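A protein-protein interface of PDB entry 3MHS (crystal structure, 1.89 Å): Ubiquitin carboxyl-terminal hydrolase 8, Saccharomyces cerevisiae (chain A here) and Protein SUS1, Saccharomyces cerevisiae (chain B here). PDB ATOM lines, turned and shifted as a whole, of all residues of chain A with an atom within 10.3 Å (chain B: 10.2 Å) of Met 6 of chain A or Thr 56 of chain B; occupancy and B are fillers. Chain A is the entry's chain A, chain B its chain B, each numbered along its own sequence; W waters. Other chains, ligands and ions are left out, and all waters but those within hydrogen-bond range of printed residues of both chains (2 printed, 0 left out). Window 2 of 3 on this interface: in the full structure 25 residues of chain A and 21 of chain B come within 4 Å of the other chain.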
ATOM      1  N   ALA A   5       3.304  14.226 -32.788  1.00  0.00           N
ATOM      2  CA  ALA A   5       3.914  12.934 -32.335  1.00  0.00           C
ATOM      3  C   ALA A   5       4.522  13.063 -30.927  1.00  0.00           C
ATOM      4  O   ALA A   5       5.739  13.172 -30.781  1.00  0.00           O
ATOM      5  CB  ALA A   5       4.982  12.486 -33.334  1.00  0.00           C
ATOM      6  N   MET A   6       3.674  13.016 -29.900  1.00  0.00           N
ATOM      7  CA  MET A   6       4.092  13.284 -28.514  1.00  0.00           C
ATOM      8  C   MET A   6       5.359  12.528 -28.049  1.00  0.00           C
ATOM      9  O   MET A   6       5.475  11.310 -28.183  1.00  0.00           O
ATOM     10  CB  MET A   6       2.921  13.036 -27.558  1.00  0.00           C
ATOM     11  CG  MET A   6       1.996  14.249 -27.404  1.00  0.00           C
ATOM     12  SD  MET A   6       2.075  15.024 -25.755  1.00  0.00           S
ATOM     13  CE  MET A   6       1.693  16.744 -26.139  1.00  0.00           C
ATOM     14  N   SER A   7       6.301  13.270 -27.481  1.00  0.00           N
ATOM     15  CA  SER A   7       7.548  12.688 -26.995  1.00  0.00           C
ATOM     16  C   SER A   7       7.502  12.319 -25.502  1.00  0.00           C
ATOM     17  O   SER A   7       6.577  12.691 -24.778  1.00  0.00           O
ATOM     18  CB  SER A   7       8.685  13.676 -27.237  1.00  0.00           C
ATOM     19  OG  SER A   7       8.337  14.936 -26.692  1.00  0.00           O
ATOM     20  N   ILE A   8       8.519  11.574 -25.075  1.00  0.00           N
ATOM     21  CA  ILE A   8       8.746  11.235 -23.680  1.00  0.00           C
ATOM     22  C   ILE A   8      10.056  11.881 -23.212  1.00  0.00           C
ATOM     23  O   ILE A   8      10.991  12.058 -23.992  1.00  0.00           O
ATOM     24  CB  ILE A   8       8.828   9.702 -23.486  1.00  0.00           C
ATOM     25  CG1 ILE A   8       7.515   9.033 -23.925  1.00  0.00           C
ATOM     26  CG2 ILE A   8       9.122   9.366 -22.029  1.00  0.00           C
ATOM     27  CD1 ILE A   8       7.698   7.689 -24.620  1.00  0.00           C
ATOM     28  N   CYS A   9      10.120  12.249 -21.937  1.00  0.00           N
ATOM     29  CA  CYS A   9      11.317  12.853 -21.383  1.00  0.00           C
ATOM     30  C   CYS A   9      12.517  11.941 -21.651  1.00  0.00           C
ATOM     31  O   CYS A   9      12.529  10.799 -21.195  1.00  0.00           O
ATOM     32  CB  CYS A   9      11.148  13.075 -19.876  1.00  0.00           C
ATOM     33  SG  CYS A   9      12.706  13.282 -19.002  1.00  0.00           S
ATOM     34  N   PRO A  10      13.512  12.427 -22.414  1.00  0.00           N
ATOM     35  CA  PRO A  10      14.636  11.527 -22.723  1.00  0.00           C
ATOM     36  C   PRO A  10      15.543  11.324 -21.520  1.00  0.00           C
ATOM     37  O   PRO A  10      16.340  10.385 -21.495  1.00  0.00           O
ATOM     38  CB  PRO A  10      15.368  12.252 -23.858  1.00  0.00           C
ATOM     39  CG  PRO A  10      15.086  13.700 -23.630  1.00  0.00           C
ATOM     40  CD  PRO A  10      13.728  13.784 -22.957  1.00  0.00           C
ATOM     41  N   GLN A  13      14.039   8.386 -19.806  1.00  0.00           N
ATOM     42  CA  GLN A  13      14.244   7.252 -20.706  1.00  0.00           C
ATOM     43  C   GLN A  13      15.671   6.753 -20.553  1.00  0.00           C
ATOM     44  O   GLN A  13      15.912   5.560 -20.543  1.00  0.00           O
ATOM     45  CB  GLN A  13      14.069   7.658 -22.172  1.00  0.00           C
ATOM     46  CG  GLN A  13      12.631   7.712 -22.682  1.00  0.00           C
ATOM     47  CD  GLN A  13      12.606   7.940 -24.183  1.00  0.00           C
ATOM     48  OE1 GLN A  13      11.565   7.819 -24.829  1.00  0.00           O
ATOM     49  NE2 GLN A  13      13.774   8.250 -24.752  1.00  0.00           N
ATOM     50  N   LEU A  99       5.780  13.565 -11.038  1.00  0.00           N
ATOM     51  CA  LEU A  99       7.237  13.619 -11.173  1.00  0.00           C
ATOM     52  C   LEU A  99       7.637  14.656 -12.227  1.00  0.00           C
ATOM     53  O   LEU A  99       7.192  14.587 -13.377  1.00  0.00           O
ATOM     54  CB  LEU A  99       7.757  12.227 -11.562  1.00  0.00           C
ATOM     55  CG  LEU A  99       9.262  12.028 -11.725  1.00  0.00           C
ATOM     56  CD1 LEU A  99       9.967  12.327 -10.425  1.00  0.00           C
ATOM     57  CD2 LEU A  99       9.568  10.618 -12.208  1.00  0.00           C
ATOM     58  N   PHE A 100       8.441  15.621 -11.804  1.00  0.00           N
ATOM     59  CA  PHE A 100       8.903  16.710 -12.649  1.00  0.00           C
ATOM     60  C   PHE A 100      10.321  16.474 -13.133  1.00  0.00           C
ATOM     61  O   PHE A 100      11.191  16.096 -12.346  1.00  0.00           O
ATOM     62  CB  PHE A 100       8.859  18.043 -11.888  1.00  0.00           C
ATOM     63  CG  PHE A 100       8.797  19.267 -12.792  1.00  0.00           C
ATOM     64  CD1 PHE A 100       7.614  19.630 -13.418  1.00  0.00           C
ATOM     65  CD2 PHE A 100       9.914  20.049 -13.004  1.00  0.00           C
ATOM     66  CE1 PHE A 100       7.549  20.757 -14.258  1.00  0.00           C
ATOM     67  CE2 PHE A 100       9.862  21.182 -13.820  1.00  0.00           C
ATOM     68  CZ  PHE A 100       8.674  21.525 -14.457  1.00  0.00           C
ATOM     69  N   CYS A 104      13.490  19.204 -18.809  1.00  0.00           N
ATOM     70  CA  CYS A 104      12.401  19.416 -19.758  1.00  0.00           C
ATOM     71  C   CYS A 104      11.565  20.603 -19.318  1.00  0.00           C
ATOM     72  O   CYS A 104      10.882  21.238 -20.135  1.00  0.00           O
ATOM     73  CB  CYS A 104      11.524  18.175 -19.860  1.00  0.00           C
ATOM     74  SG  CYS A 104      12.301  16.743 -20.697  1.00  0.00           S
ATOM     75  N   GLU A 105      11.674  20.929 -18.029  1.00  0.00           N
ATOM     76  CA  GLU A 105      10.807  21.919 -17.406  1.00  0.00           C
ATOM     77  C   GLU A 105       9.368  21.424 -17.581  1.00  0.00           C
ATOM     78  O   GLU A 105       8.446  22.208 -17.812  1.00  0.00           O
ATOM     79  CB  GLU A 105      11.036  23.320 -18.018  1.00  0.00           C
ATOM     80  CG  GLU A 105      12.429  23.920 -17.706  1.00  0.00           C
ATOM     81  CD  GLU A 105      12.935  24.938 -18.746  1.00  0.00           C
ATOM     82  OE1 GLU A 105      12.134  25.730 -19.294  1.00  0.00           O
ATOM     83  OE2 GLU A 105      14.161  24.955 -19.007  1.00  0.00           O
ATOM     84  N   ASP A 106       9.182  20.109 -17.447  1.00  0.00           N
ATOM     85  CA  ASP A 106       7.884  19.483 -17.649  1.00  0.00           C
ATOM     86  C   ASP A 106       7.674  18.262 -16.744  1.00  0.00           C
ATOM     87  O   ASP A 106       8.634  17.590 -16.363  1.00  0.00           O
ATOM     88  CB  ASP A 106       7.745  19.060 -19.120  1.00  0.00           C
ATOM     89  CG  ASP A 106       6.297  18.732 -19.524  1.00  0.00           C
ATOM     90  OD1 ASP A 106       5.334  19.112 -18.818  1.00  0.00           O
ATOM     91  OD2 ASP A 106       6.125  18.094 -20.581  1.00  0.00           O
ATOM     92  N   TYR A 107       6.419  17.970 -16.410  1.00  0.00           N
ATOM     93  CA  TYR A 107       6.114  16.724 -15.700  1.00  0.00           C
ATOM     94  C   TYR A 107       6.213  15.548 -16.652  1.00  0.00           C
ATOM     95  O   TYR A 107       6.003  15.683 -17.859  1.00  0.00           O
ATOM     96  CB  TYR A 107       4.712  16.743 -15.060  1.00  0.00           C
ATOM     97  CG  TYR A 107       4.629  17.625 -13.835  1.00  0.00           C
ATOM     98  CD1 TYR A 107       4.988  17.141 -12.568  1.00  0.00           C
ATOM     99  CD2 TYR A 107       4.193  18.945 -13.936  1.00  0.00           C
ATOM    100  CE1 TYR A 107       4.940  17.970 -11.443  1.00  0.00           C
ATOM    101  CE2 TYR A 107       4.119  19.764 -12.823  1.00  0.00           C
ATOM    102  CZ  TYR A 107       4.526  19.288 -11.584  1.00  0.00           C
ATOM    103  OH  TYR A 107       4.442  20.138 -10.493  1.00  0.00           O
ATOM    104  N   ILE A 108       6.509  14.388 -16.084  1.00  0.00           N
ATOM    105  CA  ILE A 108       6.513  13.128 -16.798  1.00  0.00           C
ATOM    106  C   ILE A 108       5.159  12.462 -16.485  1.00  0.00           C
ATOM    107  O   ILE A 108       4.972  11.891 -15.415  1.00  0.00           O
ATOM    108  CB  ILE A 108       7.715  12.266 -16.312  1.00  0.00           C
ATOM    109  CG1 ILE A 108       9.020  13.074 -16.399  1.00  0.00           C
ATOM    110  CG2 ILE A 108       7.830  10.967 -17.080  1.00  0.00           C
ATOM    111  CD1 ILE A 108      10.237  12.369 -15.796  1.00  0.00           C
ATOM    112  N   GLY A 109       4.202  12.596 -17.407  1.00  0.00           N
ATOM    113  CA  GLY A 109       2.820  12.152 -17.199  1.00  0.00           C
ATOM    114  C   GLY A 109       2.402  10.993 -18.097  1.00  0.00           C
ATOM    115  O   GLY A 109       1.393  10.375 -17.863  1.00  0.00           O
ATOM    116  N   ASN A 110       3.226  10.649 -19.085  1.00  0.00           N
ATOM    117  CA  ASN A 110       2.798   9.719 -20.147  1.00  0.00           C
ATOM    118  C   ASN A 110       3.547   8.397 -20.137  1.00  0.00           C
ATOM    119  O   ASN A 110       3.530   7.662 -21.129  1.00  0.00           O
ATOM    120  CB  ASN A 110       2.915  10.379 -21.523  1.00  0.00           C
ATOM    121  CG  ASN A 110       4.342  10.740 -21.883  1.00  0.00           C
ATOM    122  OD1 ASN A 110       5.260  10.489 -21.116  1.00  0.00           O
ATOM    123  ND2 ASN A 110       4.540  11.301 -23.086  1.00  0.00           N
ATOM    124  N   ILE A 111       4.197   8.091 -19.013  1.00  0.00           N
ATOM    125  CA  ILE A 111       4.807   6.777 -18.807  1.00  0.00           C
ATOM    126  C   ILE A 111       3.920   5.962 -17.884  1.00  0.00           C
ATOM    127  O   ILE A 111       3.785   6.282 -16.706  1.00  0.00           O
ATOM    128  CB  ILE A 111       6.253   6.868 -18.222  1.00  0.00           C
ATOM    129  CG1 ILE A 111       7.170   7.620 -19.203  1.00  0.00           C
ATOM    130  CG2 ILE A 111       6.790   5.479 -17.969  1.00  0.00           C
ATOM    131  CD1 ILE A 111       8.639   7.601 -18.861  1.00  0.00           C
ATOM    132  N   THR B  46      -7.039  26.070 -18.434  1.00  0.00           N
ATOM    133  CA  THR B  46      -5.830  25.288 -18.714  1.00  0.00           C
ATOM    134  C   THR B  46      -6.009  24.453 -19.993  1.00  0.00           C
ATOM    135  O   THR B  46      -5.114  24.425 -20.841  1.00  0.00           O
ATOM    136  CB  THR B  46      -5.388  24.386 -17.495  1.00  0.00           C
ATOM    137  OG1 THR B  46      -5.226  25.194 -16.315  1.00  0.00           O
ATOM    138  CG2 THR B  46      -4.058  23.684 -17.779  1.00  0.00           C
ATOM    139  N   LYS B  47      -7.174  23.833 -20.170  1.00  0.00           N
ATOM    140  CA  LYS B  47      -7.428  23.042 -21.366  1.00  0.00           C
ATOM    141  C   LYS B  47      -7.391  23.953 -22.606  1.00  0.00           C
ATOM    142  O   LYS B  47      -6.855  23.578 -23.643  1.00  0.00           O
ATOM    143  CB  LYS B  47      -8.789  22.362 -21.297  1.00  0.00           C
ATOM    144  CG  LYS B  47      -8.992  21.431 -20.123  1.00  0.00           C
ATOM    145  CD  LYS B  47      -8.899  19.972 -20.509  1.00  0.00           C
ATOM    146  CE  LYS B  47     -10.013  19.170 -19.845  1.00  0.00           C
ATOM    147  NZ  LYS B  47     -10.006  19.302 -18.361  1.00  0.00           N
ATOM    148  N   SER B  48      -7.973  25.144 -22.471  1.00  0.00           N
ATOM    149  CA  SER B  48      -8.021  26.133 -23.539  1.00  0.00           C
ATOM    150  C   SER B  48      -6.618  26.592 -23.954  1.00  0.00           C
ATOM    151  O   SER B  48      -6.313  26.678 -25.144  1.00  0.00           O
ATOM    152  CB  SER B  48      -8.851  27.341 -23.079  1.00  0.00           C
ATOM    153  OG  SER B  48      -9.008  28.274 -24.131  1.00  0.00           O
ATOM    154  N   GLU B  49      -5.765  26.867 -22.970  1.00  0.00           N
ATOM    155  CA  GLU B  49      -4.402  27.297 -23.243  1.00  0.00           C
ATOM    156  C   GLU B  49      -3.592  26.182 -23.887  1.00  0.00           C
ATOM    157  O   GLU B  49      -2.795  26.421 -24.800  1.00  0.00           O
ATOM    158  CB  GLU B  49      -3.736  27.783 -21.960  1.00  0.00           C
ATOM    159  CG  GLU B  49      -4.315  29.112 -21.442  1.00  0.00           C
ATOM    160  CD  GLU B  49      -4.100  30.272 -22.404  1.00  0.00           C
ATOM    161  OE1 GLU B  49      -2.977  30.434 -22.913  1.00  0.00           O
ATOM    162  OE2 GLU B  49      -5.066  31.005 -22.674  1.00  0.00           O
ATOM    163  N   MET B  50      -3.798  24.957 -23.428  1.00  0.00           N
ATOM    164  CA  MET B  50      -3.159  23.810 -24.079  1.00  0.00           C
ATOM    165  C   MET B  50      -3.584  23.713 -25.558  1.00  0.00           C
ATOM    166  O   MET B  50      -2.772  23.364 -26.420  1.00  0.00           O
ATOM    167  CB  MET B  50      -3.473  22.510 -23.328  1.00  0.00           C
ATOM    168  CG  MET B  50      -2.672  22.341 -22.036  1.00  0.00           C
ATOM    169  SD  MET B  50      -2.816  20.709 -21.243  1.00  0.00           S
ATOM    170  CE  MET B  50      -4.491  20.797 -20.627  1.00  0.00           C
ATOM    171  N   ASN B  51      -4.848  24.015 -25.853  1.00  0.00           N
ATOM    172  CA  ASN B  51      -5.334  23.931 -27.234  1.00  0.00           C
ATOM    173  C   ASN B  51      -4.838  25.076 -28.112  1.00  0.00           C
ATOM    174  O   ASN B  51      -4.526  24.867 -29.284  1.00  0.00           O
ATOM    175  CB  ASN B  51      -6.864  23.851 -27.288  1.00  0.00           C
ATOM    176  CG  ASN B  51      -7.396  22.491 -26.839  1.00  0.00           C
ATOM    177  OD1 ASN B  51      -6.800  21.446 -27.132  1.00  0.00           O
ATOM    178  ND2 ASN B  51      -8.523  22.498 -26.135  1.00  0.00           N
ATOM    179  N   ILE B  52      -4.738  26.264 -27.517  1.00  0.00           N
ATOM    180  CA  ILE B  52      -4.295  27.465 -28.210  1.00  0.00           C
ATOM    181  C   ILE B  52      -2.811  27.382 -28.510  1.00  0.00           C
ATOM    182  O   ILE B  52      -2.364  27.792 -29.575  1.00  0.00           O
ATOM    183  CB  ILE B  52      -4.535  28.720 -27.359  1.00  0.00           C
ATOM    184  CG1 ILE B  52      -6.024  29.042 -27.308  1.00  0.00           C
ATOM    185  CG2 ILE B  52      -3.790  29.917 -27.931  1.00  0.00           C
ATOM    186  CD1 ILE B  52      -6.399  29.916 -26.123  1.00  0.00           C
ATOM    187  N   ASN B  53      -2.054  26.853 -27.554  1.00  0.00           N
ATOM    188  CA  ASN B  53      -0.610  26.772 -27.687  1.00  0.00           C
ATOM    189  C   ASN B  53      -0.118  25.417 -28.195  1.00  0.00           C
ATOM    190  O   ASN B  53       1.079  25.258 -28.475  1.00  0.00           O
ATOM    191  CB  ASN B  53       0.049  27.149 -26.364  1.00  0.00           C
ATOM    192  CG  ASN B  53      -0.115  28.626 -26.047  1.00  0.00           C
ATOM    193  OD1 ASN B  53       0.495  29.466 -26.693  1.00  0.00           O
ATOM    194  ND2 ASN B  53      -0.964  28.947 -25.078  1.00  0.00           N
ATOM    195  N   GLU B  54      -1.049  24.474 -28.378  1.00  0.00           N
ATOM    196  CA  GLU B  54      -0.729  23.142 -28.922  1.00  0.00           C
ATOM    197  C   GLU B  54       0.431  22.518 -28.144  1.00  0.00           C
ATOM    198  O   GLU B  54       1.434  22.086 -28.715  1.00  0.00           O
ATOM    199  CB  GLU B  54      -0.367  23.230 -30.416  1.00  0.00           C
ATOM    200  CG  GLU B  54      -1.479  23.781 -31.306  1.00  0.00           C
ATOM    201  CD  GLU B  54      -1.122  23.774 -32.786  1.00  0.00           C
ATOM    202  OE1 GLU B  54      -1.732  24.556 -33.545  1.00  0.00           O
ATOM    203  OE2 GLU B  54      -0.230  22.999 -33.195  1.00  0.00           O
ATOM    204  N   SER B  55       0.291  22.500 -26.830  1.00  0.00           N
ATOM    205  CA  SER B  55       1.388  22.160 -25.952  1.00  0.00           C
ATOM    206  C   SER B  55       0.811  21.656 -24.645  1.00  0.00           C
ATOM    207  O   SER B  55      -0.251  22.109 -24.223  1.00  0.00           O
ATOM    208  CB  SER B  55       2.247  23.406 -25.703  1.00  0.00           C
ATOM    209  OG  SER B  55       3.284  23.162 -24.764  1.00  0.00           O
ATOM    210  N   THR B  56       1.490  20.684 -24.047  1.00  0.00           N
ATOM    211  CA  THR B  56       1.195  20.259 -22.686  1.00  0.00           C
ATOM    212  C   THR B  56       2.394  20.565 -21.780  1.00  0.00           C
ATOM    213  O   THR B  56       2.464  20.053 -20.662  1.00  0.00           O
ATOM    214  CB  THR B  56       0.859  18.739 -22.601  1.00  0.00           C
ATOM    215  OG1 THR B  56       1.966  17.961 -23.078  1.00  0.00           O
ATOM    216  CG2 THR B  56      -0.397  18.392 -23.408  1.00  0.00           C
ATOM    217  N   ASN B  57       3.334  21.397 -22.253  1.00  0.00           N
ATOM    218  CA  ASN B  57       4.504  21.760 -21.446  1.00  0.00           C
ATOM    219  C   ASN B  57       4.072  22.607 -20.267  1.00  0.00           C
ATOM    220  O   ASN B  57       3.455  23.667 -20.427  1.00  0.00           O
ATOM    221  CB  ASN B  57       5.580  22.486 -22.267  1.00  0.00           C
ATOM    222  CG  ASN B  57       6.852  22.765 -21.451  1.00  0.00           C
ATOM    223  OD1 ASN B  57       7.854  22.048 -21.570  1.00  0.00           O
ATOM    224  ND2 ASN B  57       6.813  23.802 -20.624  1.00  0.00           N
ATOM    225  N   PHE B  58       4.372  22.103 -19.070  1.00  0.00           N
ATOM    226  CA  PHE B  58       3.822  22.667 -17.846  1.00  0.00           C
ATOM    227  C   PHE B  58       4.305  24.086 -17.640  1.00  0.00           C
ATOM    228  O   PHE B  58       3.539  24.951 -17.271  1.00  0.00           O
ATOM    229  CB  PHE B  58       4.191  21.812 -16.628  1.00  0.00           C
ATOM    230  CG  PHE B  58       3.843  22.463 -15.325  1.00  0.00           C
ATOM    231  CD1 PHE B  58       2.557  22.420 -14.842  1.00  0.00           C
ATOM    232  CD2 PHE B  58       4.792  23.176 -14.624  1.00  0.00           C
ATOM    233  CE1 PHE B  58       2.226  23.076 -13.674  1.00  0.00           C
ATOM    234  CE2 PHE B  58       4.475  23.815 -13.464  1.00  0.00           C
ATOM    235  CZ  PHE B  58       3.188  23.777 -12.992  1.00  0.00           C
ATOM    236  N   THR B  59       5.585  24.326 -17.889  1.00  0.00           N
ATOM    237  CA  THR B  59       6.166  25.644 -17.642  1.00  0.00           C
ATOM    238  C   THR B  59       5.548  26.699 -18.534  1.00  0.00           C
ATOM    239  O   THR B  59       5.140  27.748 -18.040  1.00  0.00           O
ATOM    240  CB  THR B  59       7.700  25.627 -17.784  1.00  0.00           C
ATOM    241  OG1 THR B  59       8.226  24.752 -16.782  1.00  0.00           O
ATOM    242  CG2 THR B  59       8.277  27.021 -17.597  1.00  0.00           C
ATOM    243  N   GLN B  60       5.429  26.416 -19.827  1.00  0.00           N
ATOM    244  CA  GLN B  60       4.833  27.389 -20.742  1.00  0.00           C
ATOM    245  C   GLN B  60       3.319  27.543 -20.544  1.00  0.00           C
ATOM    246  O   GLN B  60       2.796  28.650 -20.662  1.00  0.00           O
ATOM    247  CB  GLN B  60       5.193  27.109 -22.208  1.00  0.00           C
ATOM    248  CG  GLN B  60       4.441  25.996 -22.890  1.00  0.00           C
ATOM    249  CD  GLN B  60       4.621  26.014 -24.405  1.00  0.00           C
ATOM    250  OE1 GLN B  60       4.053  26.859 -25.101  1.00  0.00           O
ATOM    251  NE2 GLN B  60       5.407  25.070 -24.924  1.00  0.00           N
ATOM    252  N   ILE B  61       2.613  26.462 -20.214  1.00  0.00           N
ATOM    253  CA  ILE B  61       1.183  26.576 -19.967  1.00  0.00           C
ATOM    254  C   ILE B  61       0.912  27.360 -18.673  1.00  0.00           C
ATOM    255  O   ILE B  61       0.018  28.205 -18.627  1.00  0.00           O
ATOM    256  CB  ILE B  61       0.475  25.197 -19.909  1.00  0.00           C
ATOM    257  CG1 ILE B  61       0.499  24.524 -21.284  1.00  0.00           C
ATOM    258  CG2 ILE B  61      -0.980  25.355 -19.406  1.00  0.00           C
ATOM    259  CD1 ILE B  61       0.009  25.430 -22.433  1.00  0.00           C
ATOM    260  N   LEU B  62       1.679  27.084 -17.626  1.00  0.00           N
ATOM    261  CA  LEU B  62       1.516  27.792 -16.365  1.00  0.00           C
ATOM    262  C   LEU B  62       1.711  29.299 -16.531  1.00  0.00           C
ATOM    263  O   LEU B  62       1.044  30.100 -15.871  1.00  0.00           O
ATOM    264  CB  LEU B  62       2.515  27.268 -15.334  1.00  0.00           C
ATOM    265  CG  LEU B  62       2.399  27.853 -13.915  1.00  0.00           C
ATOM    266  CD1 LEU B  62       1.091  27.384 -13.177  1.00  0.00           C
ATOM    267  CD2 LEU B  62       3.630  27.489 -13.115  1.00  0.00           C
ATOM    268  N   SER B  63       2.643  29.681 -17.397  1.00  0.00           N
ATOM    269  CA  SER B  63       2.993  31.088 -17.568  1.00  0.00           C
ATOM    270  C   SER B  63       1.795  31.918 -18.044  1.00  0.00           C
ATOM    271  O   SER B  63       1.725  33.128 -17.782  1.00  0.00           O
ATOM    272  CB  SER B  63       4.149  31.226 -18.562  1.00  0.00           C
ATOM    273  OG  SER B  63       3.702  30.983 -19.883  1.00  0.00           O
ATOM    274  N   VAL B  65      -1.608  30.560 -17.766  1.00  0.00           N
ATOM    275  CA  VAL B  65      -2.743  30.240 -16.880  1.00  0.00           C
ATOM    276  C   VAL B  65      -2.678  30.962 -15.536  1.00  0.00           C
ATOM    277  O   VAL B  65      -3.665  31.558 -15.096  1.00  0.00           O
ATOM    278  CB  VAL B  65      -2.858  28.739 -16.616  1.00  0.00           C
ATOM    279  CG1 VAL B  65      -4.014  28.456 -15.624  1.00  0.00           C
ATOM    280  CG2 VAL B  65      -3.066  28.004 -17.921  1.00  0.00           C
HETATM  281  O   HOH W   1       8.357  18.892 -22.771  1.00  0.00           O
HETATM  282  O   HOH W   2       3.388  17.621 -20.719  1.00  0.00           O
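Of chain B, only Thr 56 comes within 4 Å of Met 6 of chain A.
Of chain A, only Met 6 (3.3 Å) and Asp 106 (3.5 Å) come within 4 Å of Thr 56 of chain B.
No residue of chain B comes within 4 Å of Ala 5 of chain A.
No residue of chain B comes within 4 Å of Ser 7 of chain A.
Ser 55 of chain B touches none of the printed residues of chain A.
Of the printed residues of chain B, Cys 104 of chain A touches Asn 57.
Of the printed residues of chain B, Tyr 107 of chain A touches Phe 58.
Printed residues of chain A within 4 Å of Phe 58 of chain B: Phe 100, Asp 106 and Tyr 107.
Printed residues of chain A within 4 Å of Thr 59 of chain B: Glu 105.
Of the printed residues of chain B, Glu 105 of chain A touches Asn 57 (3.6 Å) and Thr 59 (2.8 Å).
Asn 51 of chain B touches none of the printed residues of chain A.
The nearest residue of chain B that does not touch Met 6 of chain A is Ser 55 of chain B (5.2 Å).
The backbone NH of Phe 58 of chain B sits at hydrogen-bond distance from the side-chain carboxylate of Asp 106 of chain A (3.2 Å).
The backbone carbonyl oxygen (O) of Cys 104 of chain A sits close to the side-chain amide oxygen (OD1) of Asn 57 of chain B (3.4 Å).
The backbone carbonyl oxygen (O) of Glu 105 of chain A sits at hydrogen-bond distance from the side-chain hydroxyl (OG1) of Thr 59 of chain B (2.8 Å).
Water W2 lies within hydrogen-bond range of O of Thr 56 of chain B (2.6 Å) and OD2 of Asp 106 of chain A (2.8 Å).
Water W1 lies within hydrogen-bond range of OD2 of Asp 106 of chain A and OD1 of Asn 57 of chain B.
The side-chain amide nitrogen (ND2) of Asn 57 of chain B sits close to the backbone NH (N) of Thr 59 of chain B (3.0 Å).
N of Asn 57 of chain B sits at hydrogen-bond distance from OG of Ser 55 of chain B (3.1 Å).
The side-chain amide nitrogen (ND2) of Asn 57 of chain B lies close to the backbone NH (N) of Gln 60 of chain B.
Hydrophobic or aromatic side chains of chain B within 4 Å of the printed part of chain A: Phe 58.
Printed residues of chain A that touch a printed residue of chain B: Met 6, Phe 100, Cys 104, Glu 105, Asp 106 and Tyr 107.
Among the printed residues, 9 pairs touch across the chains.
Among the printed residues, pairs that only touch across the chains: Met 6 of chain A with Thr 56 of chain B (3.3 Å), Asp 106 of chain A with Thr 56 of chain B (3.5 Å), Glu 105 of chain A with Asn 57 of chain B (3.6 Å), Tyr 107 of chain A with Phe 58 of chain B (3.7 Å), Phe 100 of chain A with Phe 58 of chain B (3.7 Å) and Asp 106 of chain A with Asn 57 of chain B (3.8 Å).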
